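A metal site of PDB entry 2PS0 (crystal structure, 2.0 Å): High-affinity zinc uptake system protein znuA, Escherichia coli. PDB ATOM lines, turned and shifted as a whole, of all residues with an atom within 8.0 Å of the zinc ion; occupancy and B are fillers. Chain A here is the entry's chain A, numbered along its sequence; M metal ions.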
ATOM      1  N   LEU A   6     -12.435  -8.246 -13.873  1.00  0.00           N
ATOM      2  CA  LEU A   6     -11.124  -7.568 -13.760  1.00  0.00           C
ATOM      3  C   LEU A   6     -10.588  -7.686 -12.345  1.00  0.00           C
ATOM      4  O   LEU A   6     -11.361  -7.741 -11.389  1.00  0.00           O
ATOM      5  CB  LEU A   6     -11.255  -6.083 -14.130  1.00  0.00           C
ATOM      6  CG  LEU A   6     -12.092  -5.723 -15.381  1.00  0.00           C
ATOM      7  CD1 LEU A   6     -12.307  -4.250 -15.465  1.00  0.00           C
ATOM      8  CD2 LEU A   6     -11.444  -6.249 -16.672  1.00  0.00           C
ATOM      9  N   SER A  32      -5.235  -6.136 -21.006  1.00  0.00           N
ATOM     10  CA  SER A  32      -5.961  -4.877 -20.910  1.00  0.00           C
ATOM     11  C   SER A  32      -7.473  -5.081 -21.036  1.00  0.00           C
ATOM     12  O   SER A  32      -7.947  -5.884 -21.872  1.00  0.00           O
ATOM     13  CB  SER A  32      -5.477  -3.902 -21.978  1.00  0.00           C
ATOM     14  OG  SER A  32      -6.283  -2.732 -21.981  1.00  0.00           O
ATOM     15  N   GLU A  33      -8.221  -4.346 -20.213  1.00  0.00           N
ATOM     16  CA  GLU A  33      -9.685  -4.360 -20.240  1.00  0.00           C
ATOM     17  C   GLU A  33     -10.238  -3.916 -21.612  1.00  0.00           C
ATOM     18  O   GLU A  33     -11.373  -4.250 -21.970  1.00  0.00           O
ATOM     19  CB  GLU A  33     -10.270  -3.515 -19.076  1.00  0.00           C
ATOM     20  CG  GLU A  33     -10.027  -1.978 -19.131  1.00  0.00           C
ATOM     21  CD  GLU A  33      -8.695  -1.517 -18.551  1.00  0.00           C
ATOM     22  OE1 GLU A  33      -8.524  -0.283 -18.316  1.00  0.00           O
ATOM     23  OE2 GLU A  33      -7.805  -2.366 -18.314  1.00  0.00           O
ATOM     24  N   HIS A  34      -9.413  -3.213 -22.398  1.00  0.00           N
ATOM     25  CA  HIS A  34      -9.825  -2.686 -23.711  1.00  0.00           C
ATOM     26  C   HIS A  34      -9.478  -3.560 -24.917  1.00  0.00           C
ATOM     27  O   HIS A  34      -9.847  -3.239 -26.065  1.00  0.00           O
ATOM     28  CB  HIS A  34      -9.242  -1.289 -23.907  1.00  0.00           C
ATOM     29  CG  HIS A  34      -9.632  -0.336 -22.826  1.00  0.00           C
ATOM     30  ND1 HIS A  34     -10.934   0.087 -22.657  1.00  0.00           N
ATOM     31  CD2 HIS A  34      -8.905   0.273 -21.871  1.00  0.00           C
ATOM     32  CE1 HIS A  34     -10.984   0.928 -21.641  1.00  0.00           C
ATOM     33  NE2 HIS A  34      -9.773   1.052 -21.142  1.00  0.00           N
ATOM     34  N   MET A  59     -17.878  -1.412 -20.800  1.00  0.00           N
ATOM     35  CA  MET A  59     -16.528  -1.653 -20.314  1.00  0.00           C
ATOM     36  C   MET A  59     -16.016  -2.991 -20.863  1.00  0.00           C
ATOM     37  O   MET A  59     -15.297  -2.988 -21.860  1.00  0.00           O
ATOM     38  CB  MET A  59     -16.466  -1.549 -18.775  1.00  0.00           C
ATOM     39  CG  MET A  59     -15.114  -1.944 -18.110  1.00  0.00           C
ATOM     40  SD  MET A  59     -13.628  -1.261 -18.867  1.00  0.00           S
ATOM     41  CE  MET A  59     -13.865   0.498 -18.591  1.00  0.00           C
ATOM     42  N   ASN A 115     -17.446   7.767 -18.204  1.00  0.00           N
ATOM     43  CA  ASN A 115     -16.253   6.978 -17.911  1.00  0.00           C
ATOM     44  C   ASN A 115     -16.632   5.713 -17.129  1.00  0.00           C
ATOM     45  O   ASN A 115     -17.385   5.790 -16.145  1.00  0.00           O
ATOM     46  CB  ASN A 115     -15.215   7.794 -17.134  1.00  0.00           C
ATOM     47  CG  ASN A 115     -13.834   7.155 -17.133  1.00  0.00           C
ATOM     48  OD1 ASN A 115     -13.649   6.053 -16.639  1.00  0.00           O
ATOM     49  ND2 ASN A 115     -12.844   7.866 -17.696  1.00  0.00           N
ATOM     50  N   MET A 116     -16.099   4.576 -17.564  1.00  0.00           N
ATOM     51  CA  MET A 116     -16.475   3.269 -17.014  1.00  0.00           C
ATOM     52  C   MET A 116     -15.384   2.607 -16.147  1.00  0.00           C
ATOM     53  O   MET A 116     -15.465   1.410 -15.859  1.00  0.00           O
ATOM     54  CB  MET A 116     -16.918   2.318 -18.138  1.00  0.00           C
ATOM     55  CG  MET A 116     -18.262   2.656 -18.762  1.00  0.00           C
ATOM     56  SD  MET A 116     -19.594   2.300 -17.593  1.00  0.00           S
ATOM     57  CE  MET A 116     -20.749   3.570 -18.105  1.00  0.00           C
ATOM     58  N   HIS A 117     -14.388   3.381 -15.720  1.00  0.00           N
ATOM     59  CA  HIS A 117     -13.344   2.810 -14.851  1.00  0.00           C
ATOM     60  C   HIS A 117     -13.784   2.927 -13.389  1.00  0.00           C
ATOM     61  O   HIS A 117     -13.165   3.634 -12.577  1.00  0.00           O
ATOM     62  CB  HIS A 117     -11.991   3.483 -15.112  1.00  0.00           C
ATOM     63  CG  HIS A 117     -11.456   3.232 -16.491  1.00  0.00           C
ATOM     64  ND1 HIS A 117     -11.838   3.990 -17.578  1.00  0.00           N
ATOM     65  CD2 HIS A 117     -10.586   2.317 -16.951  1.00  0.00           C
ATOM     66  CE1 HIS A 117     -11.221   3.545 -18.654  1.00  0.00           C
ATOM     67  NE2 HIS A 117     -10.456   2.529 -18.305  1.00  0.00           N
ATOM     68  N   TRP A 119     -14.063   0.940 -10.760  1.00  0.00           N
ATOM     69  CA  TRP A 119     -13.407   0.280  -9.632  1.00  0.00           C
ATOM     70  C   TRP A 119     -12.412   1.204  -8.905  1.00  0.00           C
ATOM     71  O   TRP A 119     -11.895   0.841  -7.850  1.00  0.00           O
ATOM     72  CB  TRP A 119     -12.716  -1.012 -10.086  1.00  0.00           C
ATOM     73  CG  TRP A 119     -11.654  -0.779 -11.131  1.00  0.00           C
ATOM     74  CD1 TRP A 119     -10.312  -0.534 -10.916  1.00  0.00           C
ATOM     75  CD2 TRP A 119     -11.833  -0.800 -12.554  1.00  0.00           C
ATOM     76  NE1 TRP A 119      -9.662  -0.409 -12.118  1.00  0.00           N
ATOM     77  CE2 TRP A 119     -10.558  -0.558 -13.138  1.00  0.00           C
ATOM     78  CE3 TRP A 119     -12.937  -0.998 -13.389  1.00  0.00           C
ATOM     79  CZ2 TRP A 119     -10.370  -0.501 -14.519  1.00  0.00           C
ATOM     80  CZ3 TRP A 119     -12.756  -0.931 -14.777  1.00  0.00           C
ATOM     81  CH2 TRP A 119     -11.472  -0.697 -15.326  1.00  0.00           C
ATOM     82  N   HIS A 181      -3.514   6.226 -20.288  1.00  0.00           N
ATOM     83  CA  HIS A 181      -4.890   6.218 -20.757  1.00  0.00           C
ATOM     84  C   HIS A 181      -5.897   6.689 -19.703  1.00  0.00           C
ATOM     85  O   HIS A 181      -5.601   6.705 -18.510  1.00  0.00           O
ATOM     86  CB  HIS A 181      -5.268   4.904 -21.453  1.00  0.00           C
ATOM     87  CG  HIS A 181      -5.917   3.874 -20.573  1.00  0.00           C
ATOM     88  ND1 HIS A 181      -5.201   2.989 -19.805  1.00  0.00           N
ATOM     89  CD2 HIS A 181      -7.221   3.530 -20.439  1.00  0.00           C
ATOM     90  CE1 HIS A 181      -6.042   2.159 -19.192  1.00  0.00           C
ATOM     91  NE2 HIS A 181      -7.268   2.468 -19.567  1.00  0.00           N
ATOM     92  N   ASP A 182      -7.071   7.099 -20.177  1.00  0.00           N
ATOM     93  CA  ASP A 182      -8.071   7.806 -19.381  1.00  0.00           C
ATOM     94  C   ASP A 182      -8.793   6.880 -18.377  1.00  0.00           C
ATOM     95  O   ASP A 182      -9.991   6.652 -18.483  1.00  0.00           O
ATOM     96  CB  ASP A 182      -9.055   8.497 -20.344  1.00  0.00           C
ATOM     97  CG  ASP A 182      -9.990   9.466 -19.642  1.00  0.00           C
ATOM     98  OD1 ASP A 182      -9.606  10.068 -18.610  1.00  0.00           O
ATOM     99  OD2 ASP A 182     -11.123   9.612 -20.130  1.00  0.00           O
ATOM    100  N   ALA A 183      -8.058   6.366 -17.396  1.00  0.00           N
ATOM    101  CA  ALA A 183      -8.584   5.346 -16.491  1.00  0.00           C
ATOM    102  C   ALA A 183      -8.817   5.828 -15.050  1.00  0.00           C
ATOM    103  O   ALA A 183      -9.402   5.100 -14.267  1.00  0.00           O
ATOM    104  CB  ALA A 183      -7.620   4.155 -16.456  1.00  0.00           C
ATOM    105  N   TYR A 184      -8.327   7.017 -14.708  1.00  0.00           N
ATOM    106  CA  TYR A 184      -8.105   7.357 -13.296  1.00  0.00           C
ATOM    107  C   TYR A 184      -9.033   8.434 -12.719  1.00  0.00           C
ATOM    108  O   TYR A 184      -8.921   8.775 -11.534  1.00  0.00           O
ATOM    109  CB  TYR A 184      -6.639   7.760 -13.085  1.00  0.00           C
ATOM    110  CG  TYR A 184      -5.652   6.762 -13.660  1.00  0.00           C
ATOM    111  CD1 TYR A 184      -5.183   5.690 -12.899  1.00  0.00           C
ATOM    112  CD2 TYR A 184      -5.209   6.881 -14.974  1.00  0.00           C
ATOM    113  CE1 TYR A 184      -4.283   4.758 -13.438  1.00  0.00           C
ATOM    114  CE2 TYR A 184      -4.324   5.958 -15.527  1.00  0.00           C
ATOM    115  CZ  TYR A 184      -3.868   4.897 -14.752  1.00  0.00           C
ATOM    116  OH  TYR A 184      -2.984   3.974 -15.305  1.00  0.00           O
ATOM    117  N   VAL A 201      -7.179   7.634 -25.162  1.00  0.00           N
ATOM    118  CA  VAL A 201      -8.440   7.226 -24.534  1.00  0.00           C
ATOM    119  C   VAL A 201      -8.423   5.710 -24.522  1.00  0.00           C
ATOM    120  O   VAL A 201      -8.458   5.078 -23.449  1.00  0.00           O
ATOM    121  CB  VAL A 201      -9.681   7.772 -25.278  1.00  0.00           C
ATOM    122  CG1 VAL A 201     -10.964   7.112 -24.761  1.00  0.00           C
ATOM    123  CG2 VAL A 201      -9.751   9.284 -25.136  1.00  0.00           C
ATOM    124  N   ASN A 202      -8.351   5.133 -25.721  1.00  0.00           N
ATOM    125  CA  ASN A 202      -8.132   3.716 -25.891  1.00  0.00           C
ATOM    126  C   ASN A 202      -6.635   3.458 -26.084  1.00  0.00           C
ATOM    127  O   ASN A 202      -6.046   3.895 -27.082  1.00  0.00           O
ATOM    128  CB  ASN A 202      -8.953   3.168 -27.080  1.00  0.00           C
ATOM    129  CG  ASN A 202     -10.457   3.143 -26.796  1.00  0.00           C
ATOM    130  OD1 ASN A 202     -10.914   2.584 -25.790  1.00  0.00           O
ATOM    131  ND2 ASN A 202     -11.224   3.757 -27.684  1.00  0.00           N
ATOM    132  N   PRO A 203      -6.005   2.765 -25.107  1.00  0.00           N
ATOM    133  CA  PRO A 203      -4.555   2.567 -25.095  1.00  0.00           C
ATOM    134  C   PRO A 203      -3.974   1.659 -26.188  1.00  0.00           C
ATOM    135  O   PRO A 203      -2.749   1.488 -26.254  1.00  0.00           O
ATOM    136  CB  PRO A 203      -4.297   1.978 -23.721  1.00  0.00           C
ATOM    137  CG  PRO A 203      -5.558   1.293 -23.367  1.00  0.00           C
ATOM    138  CD  PRO A 203      -6.642   2.135 -23.930  1.00  0.00           C
ATOM    139  N   GLU A 204      -4.833   1.074 -27.021  1.00  0.00           N
ATOM    140  CA  GLU A 204      -4.365   0.284 -28.160  1.00  0.00           C
ATOM    141  C   GLU A 204      -4.129   1.169 -29.379  1.00  0.00           C
ATOM    142  O   GLU A 204      -3.153   0.951 -30.104  1.00  0.00           O
ATOM    143  CB  GLU A 204      -5.323  -0.866 -28.512  1.00  0.00           C
ATOM    144  CG  GLU A 204      -5.418  -1.937 -27.429  1.00  0.00           C
ATOM    145  CD  GLU A 204      -6.327  -1.529 -26.271  1.00  0.00           C
ATOM    146  OE1 GLU A 204      -7.351  -0.841 -26.540  1.00  0.00           O
ATOM    147  OE2 GLU A 204      -6.029  -1.887 -25.114  1.00  0.00           O
ATOM    148  N   GLU A 230       2.117   2.673 -18.039  1.00  0.00           N
ATOM    149  CA  GLU A 230       1.295   1.608 -17.463  1.00  0.00           C
ATOM    150  C   GLU A 230       1.934   0.264 -17.837  1.00  0.00           C
ATOM    151  O   GLU A 230       2.418   0.107 -18.978  1.00  0.00           O
ATOM    152  CB  GLU A 230      -0.147   1.705 -18.000  1.00  0.00           C
ATOM    153  CG  GLU A 230      -0.880   2.970 -17.527  1.00  0.00           C
ATOM    154  CD  GLU A 230      -2.209   3.271 -18.227  1.00  0.00           C
ATOM    155  OE1 GLU A 230      -2.650   2.465 -19.087  1.00  0.00           O
ATOM    156  OE2 GLU A 230      -2.808   4.319 -17.893  1.00  0.00           O
ATOM    157  N   PHE A 233       1.257  -1.749 -21.201  1.00  0.00           N
ATOM    158  CA  PHE A 233       1.638  -1.153 -22.475  1.00  0.00           C
ATOM    159  C   PHE A 233       3.107  -0.743 -22.514  1.00  0.00           C
ATOM    160  O   PHE A 233       3.649  -0.268 -21.518  1.00  0.00           O
ATOM    161  CB  PHE A 233       0.706   0.027 -22.826  1.00  0.00           C
ATOM    162  CG  PHE A 233      -0.727  -0.400 -22.966  1.00  0.00           C
ATOM    163  CD1 PHE A 233      -1.159  -1.006 -24.144  1.00  0.00           C
ATOM    164  CD2 PHE A 233      -1.623  -0.243 -21.914  1.00  0.00           C
ATOM    165  CE1 PHE A 233      -2.471  -1.434 -24.273  1.00  0.00           C
ATOM    166  CE2 PHE A 233      -2.928  -0.692 -22.034  1.00  0.00           C
ATOM    167  CZ  PHE A 233      -3.359  -1.297 -23.212  1.00  0.00           C
ATOM    168  N   PRO A 254      -3.742   0.583 -13.171  1.00  0.00           N
ATOM    169  CA  PRO A 254      -5.162   0.692 -12.842  1.00  0.00           C
ATOM    170  C   PRO A 254      -5.782  -0.689 -12.587  1.00  0.00           C
ATOM    171  O   PRO A 254      -6.928  -0.766 -12.149  1.00  0.00           O
ATOM    172  CB  PRO A 254      -5.763   1.340 -14.081  1.00  0.00           C
ATOM    173  CG  PRO A 254      -4.861   0.893 -15.228  1.00  0.00           C
ATOM    174  CD  PRO A 254      -3.477   0.754 -14.604  1.00  0.00           C
ATOM    175  N   LEU A 255      -5.010  -1.748 -12.798  1.00  0.00           N
ATOM    176  CA  LEU A 255      -5.481  -3.131 -12.640  1.00  0.00           C
ATOM    177  C   LEU A 255      -4.831  -3.906 -11.465  1.00  0.00           C
ATOM    178  O   LEU A 255      -5.144  -5.075 -11.246  1.00  0.00           O
ATOM    179  CB  LEU A 255      -5.375  -3.882 -13.975  1.00  0.00           C
ATOM    180  CG  LEU A 255      -6.292  -3.378 -15.111  1.00  0.00           C
ATOM    181  CD1 LEU A 255      -5.977  -4.082 -16.431  1.00  0.00           C
ATOM    182  CD2 LEU A 255      -7.796  -3.548 -14.771  1.00  0.00           C
HETATM  183 ZN    ZN M   1      -8.992   1.422 -19.293  1.00  0.00          ZN
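A ring nitrogen (ND1) of His 181 sits at hydrogen-bond distance from the side-chain carboxylate (OE1) of Glu 230, at 2.7 Å.
The backbone NH of His 34 sits close to the side-chain hydroxyl of Ser 32.
O of Asp 182 sits close to ND1 of His 117, 3.4 Å away.
ND1 of His 117 lies within hydrogen-bond range of OD1 of Asn 115.
Of the 21 residues printed, 4 come within 4 Å of the zinc ion.
The side-chain carboxylate (OE1) of Glu 33 binds the zinc ion.
The zinc ion is bound by a ring nitrogen (NE2) of His 181 (2.0 Å).
The zinc ion is bound by NE2 of His 34, at 2.0 Å.
NE2 of His 117 is bound to the zinc ion (2.1 Å).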
